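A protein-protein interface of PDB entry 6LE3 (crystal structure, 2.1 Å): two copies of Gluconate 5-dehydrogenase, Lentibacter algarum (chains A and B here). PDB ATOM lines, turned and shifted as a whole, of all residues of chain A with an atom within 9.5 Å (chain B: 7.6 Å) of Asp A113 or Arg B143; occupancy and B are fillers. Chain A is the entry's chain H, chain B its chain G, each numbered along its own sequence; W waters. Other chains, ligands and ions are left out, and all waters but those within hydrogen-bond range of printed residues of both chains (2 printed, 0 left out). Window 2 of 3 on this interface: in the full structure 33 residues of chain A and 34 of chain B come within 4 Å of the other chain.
Of the 21 printed residues of chain B, 5 touch a printed residue of chain A. Printed residues of chain B that touch a printed residue of chain A: Phe B132, Lys B136, Arg B143, Ala B185 and Trp B186. Hydrophobic or aromatic side chains of chain B that line the printed part of chain A: Phe B132, Ala B185 and Trp B186. Among the printed residues, Asp or Glu carboxylates within 4 Å of a Lys or Arg side-chain nitrogen of the other chain: Asp A113 with Arg B143.
The guanidinium group (NE) of Arg B143 is in salt-bridge range of the side-chain carboxylate (OD2) of Asp B189 (3.0 Å).
O of Ala A112 touches CZ of Phe B132 (3.4 Å). CE of Lys B136 touches O of Ala A112, 3.4 Å away. Ala A112 touches Ala B185. Trp B186 touches Ala A112 (CZ2 to CB, 3.7 Å). Asp A113 touches Lys B136. Val A115 touches Phe B132 (CB to CZ, 3.7 Å). Lys B136 touches Val A115 (CE to O, 3.4 Å). Ile A166 touches Phe B132.
Water W2 lies within hydrogen-bond range of the side-chain carboxylate of Asp A113 (2.6 Å) and the backbone carbonyl oxygen of Lys B136 (3.0 Å). Water W1 bridges the side-chain amino group of Lys B136 and the backbone carbonyl oxygen of Asp A113.
Of chain B, only Lys B136 (3.7 Å), Arg B143 (2.7 Å) and Trp B186 (2.9 Å) come within 4 Å of Asp A113. Of chain A, only Asp A113 comes within 4 Å of Arg B143. Of the printed residues of chain B, Ala A112 touches Phe B132, Lys B136, Ala B185 and Trp B186. No residue of chain A comes within 4 Å of Pro B140. Of the printed residues of chain A, Trp B186 touches Ala A112 and Asp A113. Of the printed residues of chain A, Ala B185 touches Ala A112 (3.6 Å). Of the printed residues of chain A, Lys B136 touches Ala A112, Asp A113 and Val A115. Ala B137 touches none of the printed residues of chain A. Glu B141 touches none of the printed residues of chain A. The nearest residue of chain B that does not touch Asp A113 is Val B139 (4.4 Å).
No position is printed for both chains. Of the 10 pairs that touch across the chains among the printed residues, none has its exchanged pair printed and touching as well.
OD2 of Asp A113 is in salt-bridge range of NH2 of Arg B143, at 2.7 Å. NE1 of Trp B186 sits at hydrogen-bond distance from OD1 of Asp A113 (2.9 Å).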
ATOM      1  N   ARG A 109       4.666 -27.023  12.753  1.00  0.00           N
ATOM      2  CA  ARG A 109       4.460 -27.041  11.308  1.00  0.00           C
ATOM      3  C   ARG A 109       5.030 -25.810  10.596  1.00  0.00           C
ATOM      4  O   ARG A 109       4.710 -25.570   9.432  1.00  0.00           O
ATOM      5  CB  ARG A 109       2.974 -27.229  10.967  1.00  0.00           C
ATOM      6  CG  ARG A 109       2.447 -28.578  11.462  1.00  0.00           C
ATOM      7  CD  ARG A 109       1.118 -28.987  10.820  1.00  0.00           C
ATOM      8  NE  ARG A 109       1.079 -30.424  10.556  1.00  0.00           N
ATOM      9  CZ  ARG A 109       1.036 -31.368  11.495  1.00  0.00           C
ATOM     10  NH1 ARG A 109       1.007 -31.044  12.787  1.00  0.00           N
ATOM     11  NH2 ARG A 109       1.016 -32.646  11.141  1.00  0.00           N
ATOM     12  N   GLU A 110       5.907 -25.045  11.251  1.00  0.00           N
ATOM     13  CA  GLU A 110       6.558 -23.913  10.595  1.00  0.00           C
ATOM     14  C   GLU A 110       7.604 -24.418   9.599  1.00  0.00           C
ATOM     15  O   GLU A 110       8.557 -25.107   9.980  1.00  0.00           O
ATOM     16  CB  GLU A 110       7.228 -22.999  11.624  1.00  0.00           C
ATOM     17  CG  GLU A 110       6.315 -22.158  12.479  1.00  0.00           C
ATOM     18  CD  GLU A 110       7.093 -21.355  13.541  1.00  0.00           C
ATOM     19  OE1 GLU A 110       8.287 -21.660  13.791  1.00  0.00           O
ATOM     20  OE2 GLU A 110       6.506 -20.429  14.143  1.00  0.00           O
ATOM     21  N   ALA A 111       7.429 -24.087   8.326  1.00  0.00           N
ATOM     22  CA  ALA A 111       8.447 -24.389   7.334  1.00  0.00           C
ATOM     23  C   ALA A 111       9.708 -23.582   7.636  1.00  0.00           C
ATOM     24  O   ALA A 111       9.672 -22.610   8.383  1.00  0.00           O
ATOM     25  CB  ALA A 111       7.919 -24.095   5.922  1.00  0.00           C
ATOM     26  N   ALA A 112      10.835 -24.016   7.051  1.00  0.00           N
ATOM     27  CA  ALA A 112      12.159 -23.473   7.382  1.00  0.00           C
ATOM     28  C   ALA A 112      12.224 -21.943   7.316  1.00  0.00           C
ATOM     29  O   ALA A 112      12.693 -21.291   8.258  1.00  0.00           O
ATOM     30  CB  ALA A 112      13.215 -24.089   6.464  1.00  0.00           C
ATOM     31  N   ASP A 113      11.784 -21.349   6.203  1.00  0.00           N
ATOM     32  CA  ASP A 113      11.879 -19.901   6.060  1.00  0.00           C
ATOM     33  C   ASP A 113      10.847 -19.145   6.877  1.00  0.00           C
ATOM     34  O   ASP A 113      10.897 -17.912   6.903  1.00  0.00           O
ATOM     35  CB  ASP A 113      11.753 -19.503   4.597  1.00  0.00           C
ATOM     36  CG  ASP A 113      12.813 -20.131   3.760  1.00  0.00           C
ATOM     37  OD1 ASP A 113      13.940 -20.251   4.278  1.00  0.00           O
ATOM     38  OD2 ASP A 113      12.531 -20.535   2.610  1.00  0.00           O
ATOM     39  N   ASP A 114       9.920 -19.836   7.533  1.00  0.00           N
ATOM     40  CA  ASP A 114       8.950 -19.193   8.411  1.00  0.00           C
ATOM     41  C   ASP A 114       9.194 -19.479   9.886  1.00  0.00           C
ATOM     42  O   ASP A 114       8.364 -19.101  10.718  1.00  0.00           O
ATOM     43  CB  ASP A 114       7.524 -19.617   8.036  1.00  0.00           C
ATOM     44  CG  ASP A 114       7.238 -19.454   6.548  1.00  0.00           C
ATOM     45  OD1 ASP A 114       7.636 -18.422   5.959  1.00  0.00           O
ATOM     46  OD2 ASP A 114       6.626 -20.369   5.967  1.00  0.00           O
ATOM     47  N   VAL A 115      10.267 -20.187  10.239  1.00  0.00           N
ATOM     48  CA  VAL A 115      10.453 -20.570  11.633  1.00  0.00           C
ATOM     49  C   VAL A 115      10.673 -19.331  12.488  1.00  0.00           C
ATOM     50  O   VAL A 115      11.446 -18.436  12.132  1.00  0.00           O
ATOM     51  CB  VAL A 115      11.613 -21.562  11.786  1.00  0.00           C
ATOM     52  CG1 VAL A 115      11.929 -21.766  13.275  1.00  0.00           C
ATOM     53  CG2 VAL A 115      11.251 -22.872  11.123  1.00  0.00           C
ATOM     54  N   THR A 116       9.984 -19.273  13.618  1.00  0.00           N
ATOM     55  CA  THR A 116      10.183 -18.220  14.600  1.00  0.00           C
ATOM     56  C   THR A 116      11.009 -18.754  15.761  1.00  0.00           C
ATOM     57  O   THR A 116      11.085 -19.965  15.992  1.00  0.00           O
ATOM     58  CB  THR A 116       8.840 -17.680  15.093  1.00  0.00           C
ATOM     59  OG1 THR A 116       8.060 -18.757  15.633  1.00  0.00           O
ATOM     60  CG2 THR A 116       8.097 -17.026  13.923  1.00  0.00           C
ATOM     61  N   GLY A 164       7.181 -28.668   6.406  1.00  0.00           N
ATOM     62  CA  GLY A 164       6.901 -28.001   7.663  1.00  0.00           C
ATOM     63  C   GLY A 164       7.437 -28.662   8.927  1.00  0.00           C
ATOM     64  O   GLY A 164       7.005 -28.298  10.024  1.00  0.00           O
ATOM     65  N   GLY A 165       8.375 -29.602   8.823  1.00  0.00           N
ATOM     66  CA  GLY A 165       8.796 -30.315  10.018  1.00  0.00           C
ATOM     67  C   GLY A 165      10.210 -30.061  10.515  1.00  0.00           C
ATOM     68  O   GLY A 165      10.726 -30.887  11.260  1.00  0.00           O
ATOM     69  N   ILE A 166      10.839 -28.928  10.168  1.00  0.00           N
ATOM     70  CA  ILE A 166      12.285 -28.784  10.379  1.00  0.00           C
ATOM     71  C   ILE A 166      12.648 -28.816  11.868  1.00  0.00           C
ATOM     72  O   ILE A 166      13.568 -29.542  12.279  1.00  0.00           O
ATOM     73  CB  ILE A 166      12.822 -27.524   9.669  1.00  0.00           C
ATOM     74  CG1 ILE A 166      14.339 -27.414   9.835  1.00  0.00           C
ATOM     75  CG2 ILE A 166      12.112 -26.258  10.122  1.00  0.00           C
ATOM     76  CD1 ILE A 166      15.062 -26.954   8.542  1.00  0.00           C
ATOM     77  N   ALA A 167      11.952 -28.034  12.701  1.00  0.00           N
ATOM     78  CA  ALA A 167      12.217 -28.083  14.144  1.00  0.00           C
ATOM     79  C   ALA A 167      11.847 -29.443  14.717  1.00  0.00           C
ATOM     80  O   ALA A 167      12.585 -30.021  15.536  1.00  0.00           O
ATOM     81  CB  ALA A 167      11.444 -26.982  14.877  1.00  0.00           C
ATOM     82  N   PHE B 132      20.947 -23.646  12.291  1.00  0.00           N
ATOM     83  CA  PHE B 132      19.688 -23.407  11.602  1.00  0.00           C
ATOM     84  C   PHE B 132      19.447 -21.920  11.384  1.00  0.00           C
ATOM     85  O   PHE B 132      19.155 -21.493  10.266  1.00  0.00           O
ATOM     86  CB  PHE B 132      18.493 -23.992  12.340  1.00  0.00           C
ATOM     87  CG  PHE B 132      17.192 -23.553  11.717  1.00  0.00           C
ATOM     88  CD1 PHE B 132      16.806 -24.054  10.479  1.00  0.00           C
ATOM     89  CD2 PHE B 132      16.422 -22.551  12.299  1.00  0.00           C
ATOM     90  CE1 PHE B 132      15.623 -23.609   9.861  1.00  0.00           C
ATOM     91  CE2 PHE B 132      15.245 -22.097  11.683  1.00  0.00           C
ATOM     92  CZ  PHE B 132      14.846 -22.641  10.461  1.00  0.00           C
ATOM     93  N   SER B 135      21.987 -20.423   8.876  1.00  0.00           N
ATOM     94  CA  SER B 135      21.656 -20.834   7.516  1.00  0.00           C
ATOM     95  C   SER B 135      20.425 -20.101   7.010  1.00  0.00           C
ATOM     96  O   SER B 135      20.360 -19.739   5.834  1.00  0.00           O
ATOM     97  CB  SER B 135      21.392 -22.344   7.456  1.00  0.00           C
ATOM     98  OG  SER B 135      22.448 -23.108   7.998  1.00  0.00           O
ATOM     99  N   LYS B 136      19.401 -19.979   7.864  1.00  0.00           N
ATOM    100  CA  LYS B 136      18.150 -19.329   7.489  1.00  0.00           C
ATOM    101  C   LYS B 136      18.381 -17.883   7.091  1.00  0.00           C
ATOM    102  O   LYS B 136      17.774 -17.389   6.134  1.00  0.00           O
ATOM    103  CB  LYS B 136      17.156 -19.409   8.646  1.00  0.00           C
ATOM    104  CG  LYS B 136      15.780 -18.810   8.363  1.00  0.00           C
ATOM    105  CD  LYS B 136      14.884 -18.970   9.616  1.00  0.00           C
ATOM    106  CE  LYS B 136      13.558 -18.202   9.511  1.00  0.00           C
ATOM    107  NZ  LYS B 136      13.765 -16.728   9.678  1.00  0.00           N
ATOM    108  N   ALA B 137      19.242 -17.186   7.829  1.00  0.00           N
ATOM    109  CA  ALA B 137      19.590 -15.815   7.465  1.00  0.00           C
ATOM    110  C   ALA B 137      20.262 -15.751   6.101  1.00  0.00           C
ATOM    111  O   ALA B 137      20.080 -14.779   5.365  1.00  0.00           O
ATOM    112  CB  ALA B 137      20.511 -15.209   8.523  1.00  0.00           C
ATOM    113  N   PHE B 138      21.074 -16.761   5.754  1.00  0.00           N
ATOM    114  CA  PHE B 138      21.831 -16.651   4.505  1.00  0.00           C
ATOM    115  C   PHE B 138      21.151 -17.271   3.284  1.00  0.00           C
ATOM    116  O   PHE B 138      21.572 -17.000   2.154  1.00  0.00           O
ATOM    117  CB  PHE B 138      23.215 -17.272   4.678  1.00  0.00           C
ATOM    118  CG  PHE B 138      24.126 -16.455   5.549  1.00  0.00           C
ATOM    119  CD1 PHE B 138      24.362 -15.111   5.256  1.00  0.00           C
ATOM    120  CD2 PHE B 138      24.738 -17.016   6.653  1.00  0.00           C
ATOM    121  CE1 PHE B 138      25.211 -14.342   6.045  1.00  0.00           C
ATOM    122  CE2 PHE B 138      25.587 -16.263   7.447  1.00  0.00           C
ATOM    123  CZ  PHE B 138      25.825 -14.916   7.145  1.00  0.00           C
ATOM    124  N   VAL B 139      20.131 -18.102   3.480  1.00  0.00           N
ATOM    125  CA  VAL B 139      19.523 -18.807   2.345  1.00  0.00           C
ATOM    126  C   VAL B 139      18.959 -17.860   1.288  1.00  0.00           C
ATOM    127  O   VAL B 139      19.143 -18.134   0.094  1.00  0.00           O
ATOM    128  CB  VAL B 139      18.489 -19.825   2.855  1.00  0.00           C
ATOM    129  CG1 VAL B 139      17.494 -20.181   1.763  1.00  0.00           C
ATOM    130  CG2 VAL B 139      19.179 -21.092   3.342  1.00  0.00           C
ATOM    131  N   PRO B 140      18.282 -16.745   1.629  1.00  0.00           N
ATOM    132  CA  PRO B 140      17.681 -15.896   0.568  1.00  0.00           C
ATOM    133  C   PRO B 140      18.624 -15.424  -0.535  1.00  0.00           C
ATOM    134  O   PRO B 140      18.221 -15.422  -1.708  1.00  0.00           O
ATOM    135  CB  PRO B 140      17.110 -14.720   1.365  1.00  0.00           C
ATOM    136  CG  PRO B 140      16.697 -15.358   2.667  1.00  0.00           C
ATOM    137  CD  PRO B 140      17.813 -16.333   2.969  1.00  0.00           C
ATOM    138  N   GLU B 141      19.860 -15.024  -0.209  1.00  0.00           N
ATOM    139  CA  GLU B 141      20.787 -14.605  -1.263  1.00  0.00           C
ATOM    140  C   GLU B 141      21.287 -15.796  -2.079  1.00  0.00           C
ATOM    141  O   GLU B 141      21.530 -15.663  -3.289  1.00  0.00           O
ATOM    142  CB  GLU B 141      21.967 -13.825  -0.674  1.00  0.00           C
ATOM    143  CG  GLU B 141      21.711 -12.322  -0.391  1.00  0.00           C
ATOM    144  CD  GLU B 141      20.832 -11.610  -1.438  1.00  0.00           C
ATOM    145  OE1 GLU B 141      21.139 -11.659  -2.653  1.00  0.00           O
ATOM    146  OE2 GLU B 141      19.830 -10.982  -1.026  1.00  0.00           O
ATOM    147  N   MET B 142      21.439 -16.965  -1.444  1.00  0.00           N
ATOM    148  CA  MET B 142      21.791 -18.170  -2.192  1.00  0.00           C
ATOM    149  C   MET B 142      20.706 -18.487  -3.204  1.00  0.00           C
ATOM    150  O   MET B 142      20.992 -18.774  -4.372  1.00  0.00           O
ATOM    151  CB  MET B 142      21.964 -19.359  -1.247  1.00  0.00           C
ATOM    152  CG  MET B 142      23.071 -19.238  -0.226  1.00  0.00           C
ATOM    153  SD  MET B 142      23.126 -20.767   0.702  1.00  0.00           S
ATOM    154  CE  MET B 142      24.538 -20.503   1.792  1.00  0.00           C
ATOM    155  N   ARG B 143      19.447 -18.426  -2.753  1.00  0.00           N
ATOM    156  CA  ARG B 143      18.298 -18.682  -3.607  1.00  0.00           C
ATOM    157  C   ARG B 143      18.219 -17.681  -4.747  1.00  0.00           C
ATOM    158  O   ARG B 143      17.843 -18.041  -5.866  1.00  0.00           O
ATOM    159  CB  ARG B 143      17.014 -18.643  -2.782  1.00  0.00           C
ATOM    160  CG  ARG B 143      15.754 -18.655  -3.623  1.00  0.00           C
ATOM    161  CD  ARG B 143      14.545 -18.373  -2.764  1.00  0.00           C
ATOM    162  NE  ARG B 143      14.372 -19.386  -1.726  1.00  0.00           N
ATOM    163  CZ  ARG B 143      14.170 -19.132  -0.437  1.00  0.00           C
ATOM    164  NH1 ARG B 143      14.091 -17.880  -0.003  1.00  0.00           N
ATOM    165  NH2 ARG B 143      14.033 -20.143   0.418  1.00  0.00           N
ATOM    166  N   LYS B 144      18.552 -16.414  -4.483  1.00  0.00           N
ATOM    167  CA  LYS B 144      18.577 -15.448  -5.575  1.00  0.00           C
ATOM    168  C   LYS B 144      19.630 -15.828  -6.608  1.00  0.00           C
ATOM    169  O   LYS B 144      19.375 -15.748  -7.815  1.00  0.00           O
ATOM    170  CB  LYS B 144      18.829 -14.038  -5.040  1.00  0.00           C
ATOM    171  CG  LYS B 144      17.701 -13.524  -4.136  1.00  0.00           C
ATOM    172  CD  LYS B 144      17.624 -11.999  -4.097  1.00  0.00           C
ATOM    173  CE  LYS B 144      16.582 -11.535  -3.076  1.00  0.00           C
ATOM    174  NZ  LYS B 144      16.727 -10.091  -2.712  1.00  0.00           N
ATOM    175  N   LYS B 145      20.808 -16.278  -6.151  1.00  0.00           N
ATOM    176  CA  LYS B 145      21.796 -16.822  -7.077  1.00  0.00           C
ATOM    177  C   LYS B 145      21.449 -18.222  -7.584  1.00  0.00           C
ATOM    178  O   LYS B 145      22.009 -18.652  -8.600  1.00  0.00           O
ATOM    179  CB  LYS B 145      23.181 -16.858  -6.417  1.00  0.00           C
ATOM    180  CG  LYS B 145      23.576 -15.574  -5.714  1.00  0.00           C
ATOM    181  CD  LYS B 145      25.066 -15.516  -5.439  1.00  0.00           C
ATOM    182  CE  LYS B 145      25.631 -14.189  -5.923  1.00  0.00           C
ATOM    183  NZ  LYS B 145      25.338 -13.952  -7.369  1.00  0.00           N
ATOM    184  N   GLY B 146      20.549 -18.947  -6.919  1.00  0.00           N
ATOM    185  CA  GLY B 146      20.278 -20.318  -7.327  1.00  0.00           C
ATOM    186  C   GLY B 146      21.370 -21.336  -7.026  1.00  0.00           C
ATOM    187  O   GLY B 146      21.387 -22.418  -7.624  1.00  0.00           O
ATOM    188  N   TRP B 147      22.265 -21.045  -6.091  1.00  0.00           N
ATOM    189  CA  TRP B 147      23.383 -21.938  -5.808  1.00  0.00           C
ATOM    190  C   TRP B 147      23.806 -21.721  -4.364  1.00  0.00           C
ATOM    191  O   TRP B 147      23.885 -20.579  -3.911  1.00  0.00           O
ATOM    192  CB  TRP B 147      24.561 -21.672  -6.750  1.00  0.00           C
ATOM    193  CG  TRP B 147      25.642 -22.725  -6.721  1.00  0.00           C
ATOM    194  CD1 TRP B 147      25.785 -23.786  -7.584  1.00  0.00           C
ATOM    195  CD2 TRP B 147      26.724 -22.829  -5.779  1.00  0.00           C
ATOM    196  NE1 TRP B 147      26.892 -24.529  -7.242  1.00  0.00           N
ATOM    197  CE2 TRP B 147      27.484 -23.970  -6.139  1.00  0.00           C
ATOM    198  CE3 TRP B 147      27.121 -22.079  -4.662  1.00  0.00           C
ATOM    199  CZ2 TRP B 147      28.621 -24.366  -5.428  1.00  0.00           C
ATOM    200  CZ3 TRP B 147      28.263 -22.474  -3.964  1.00  0.00           C
ATOM    201  CH2 TRP B 147      28.998 -23.600  -4.353  1.00  0.00           C
ATOM    202  N   GLY B 148      24.042 -22.819  -3.642  1.00  0.00           N
ATOM    203  CA  GLY B 148      24.432 -22.740  -2.247  1.00  0.00           C
ATOM    204  C   GLY B 148      24.919 -24.067  -1.707  1.00  0.00           C
ATOM    205  O   GLY B 148      24.491 -25.128  -2.164  1.00  0.00           O
ATOM    206  N   ALA B 185      13.744 -28.409   2.475  1.00  0.00           N
ATOM    207  CA  ALA B 185      13.268 -27.034   2.355  1.00  0.00           C
ATOM    208  C   ALA B 185      13.930 -26.284   1.206  1.00  0.00           C
ATOM    209  O   ALA B 185      13.244 -25.576   0.461  1.00  0.00           O
ATOM    210  CB  ALA B 185      13.497 -26.271   3.662  1.00  0.00           C
ATOM    211  N   TRP B 186      15.254 -26.424   1.038  1.00  0.00           N
ATOM    212  CA  TRP B 186      16.016 -25.472   0.246  1.00  0.00           C
ATOM    213  C   TRP B 186      16.679 -26.051  -0.993  1.00  0.00           C
ATOM    214  O   TRP B 186      17.036 -25.272  -1.877  1.00  0.00           O
ATOM    215  CB  TRP B 186      17.117 -24.803   1.103  1.00  0.00           C
ATOM    216  CG  TRP B 186      16.575 -24.011   2.269  1.00  0.00           C
ATOM    217  CD1 TRP B 186      15.444 -23.242   2.281  1.00  0.00           C
ATOM    218  CD2 TRP B 186      17.150 -23.891   3.581  1.00  0.00           C
ATOM    219  NE1 TRP B 186      15.267 -22.672   3.522  1.00  0.00           N
ATOM    220  CE2 TRP B 186      16.304 -23.043   4.334  1.00  0.00           C
ATOM    221  CE3 TRP B 186      18.283 -24.429   4.196  1.00  0.00           C
ATOM    222  CZ2 TRP B 186      16.557 -22.725   5.669  1.00  0.00           C
ATOM    223  CZ3 TRP B 186      18.534 -24.105   5.518  1.00  0.00           C
ATOM    224  CH2 TRP B 186      17.675 -23.256   6.240  1.00  0.00           C
ATOM    225  N   PRO B 188      15.463 -27.437  -3.640  1.00  0.00           N
ATOM    226  CA  PRO B 188      14.848 -27.069  -4.928  1.00  0.00           C
ATOM    227  C   PRO B 188      15.367 -25.759  -5.503  1.00  0.00           C
ATOM    228  O   PRO B 188      15.181 -25.503  -6.702  1.00  0.00           O
ATOM    229  CB  PRO B 188      13.353 -26.965  -4.595  1.00  0.00           C
ATOM    230  CG  PRO B 188      13.166 -27.804  -3.411  1.00  0.00           C
ATOM    231  CD  PRO B 188      14.436 -27.704  -2.617  1.00  0.00           C
ATOM    232  N   ASP B 189      16.005 -24.922  -4.689  1.00  0.00           N
ATOM    233  CA  ASP B 189      16.496 -23.618  -5.103  1.00  0.00           C
ATOM    234  C   ASP B 189      17.991 -23.648  -5.409  1.00  0.00           C
ATOM    235  O   ASP B 189      18.625 -22.587  -5.520  1.00  0.00           O
ATOM    236  CB  ASP B 189      16.188 -22.565  -4.026  1.00  0.00           C
ATOM    237  CG  ASP B 189      14.680 -22.295  -3.868  1.00  0.00           C
ATOM    238  OD1 ASP B 189      13.962 -22.203  -4.892  1.00  0.00           O
ATOM    239  OD2 ASP B 189      14.211 -22.176  -2.712  1.00  0.00           O
ATOM    240  N   GLY B 190      18.572 -24.841  -5.525  1.00  0.00           N
ATOM    241  CA  GLY B 190      19.990 -24.969  -5.787  1.00  0.00           C
ATOM    242  C   GLY B 190      20.887 -24.970  -4.566  1.00  0.00           C
ATOM    243  O   GLY B 190      22.109 -24.885  -4.724  1.00  0.00           O
ATOM    244  N   ILE B 191      20.331 -25.045  -3.360  1.00  0.00           N
ATOM    245  CA  ILE B 191      21.108 -25.073  -2.121  1.00  0.00           C
ATOM    246  C   ILE B 191      21.165 -26.506  -1.604  1.00  0.00           C
ATOM    247  O   ILE B 191      20.144 -27.053  -1.180  1.00  0.00           O
ATOM    248  CB  ILE B 191      20.498 -24.148  -1.065  1.00  0.00           C
ATOM    249  CG1 ILE B 191      20.617 -22.681  -1.531  1.00  0.00           C
ATOM    250  CG2 ILE B 191      21.196 -24.375   0.253  1.00  0.00           C
ATOM    251  CD1 ILE B 191      19.344 -21.858  -1.399  1.00  0.00           C
HETATM  252  O   HOH W   1      11.041 -16.054   9.249  1.00  0.00           O
HETATM  253  O   HOH W   2      15.430 -18.078   4.333  1.00  0.00           O
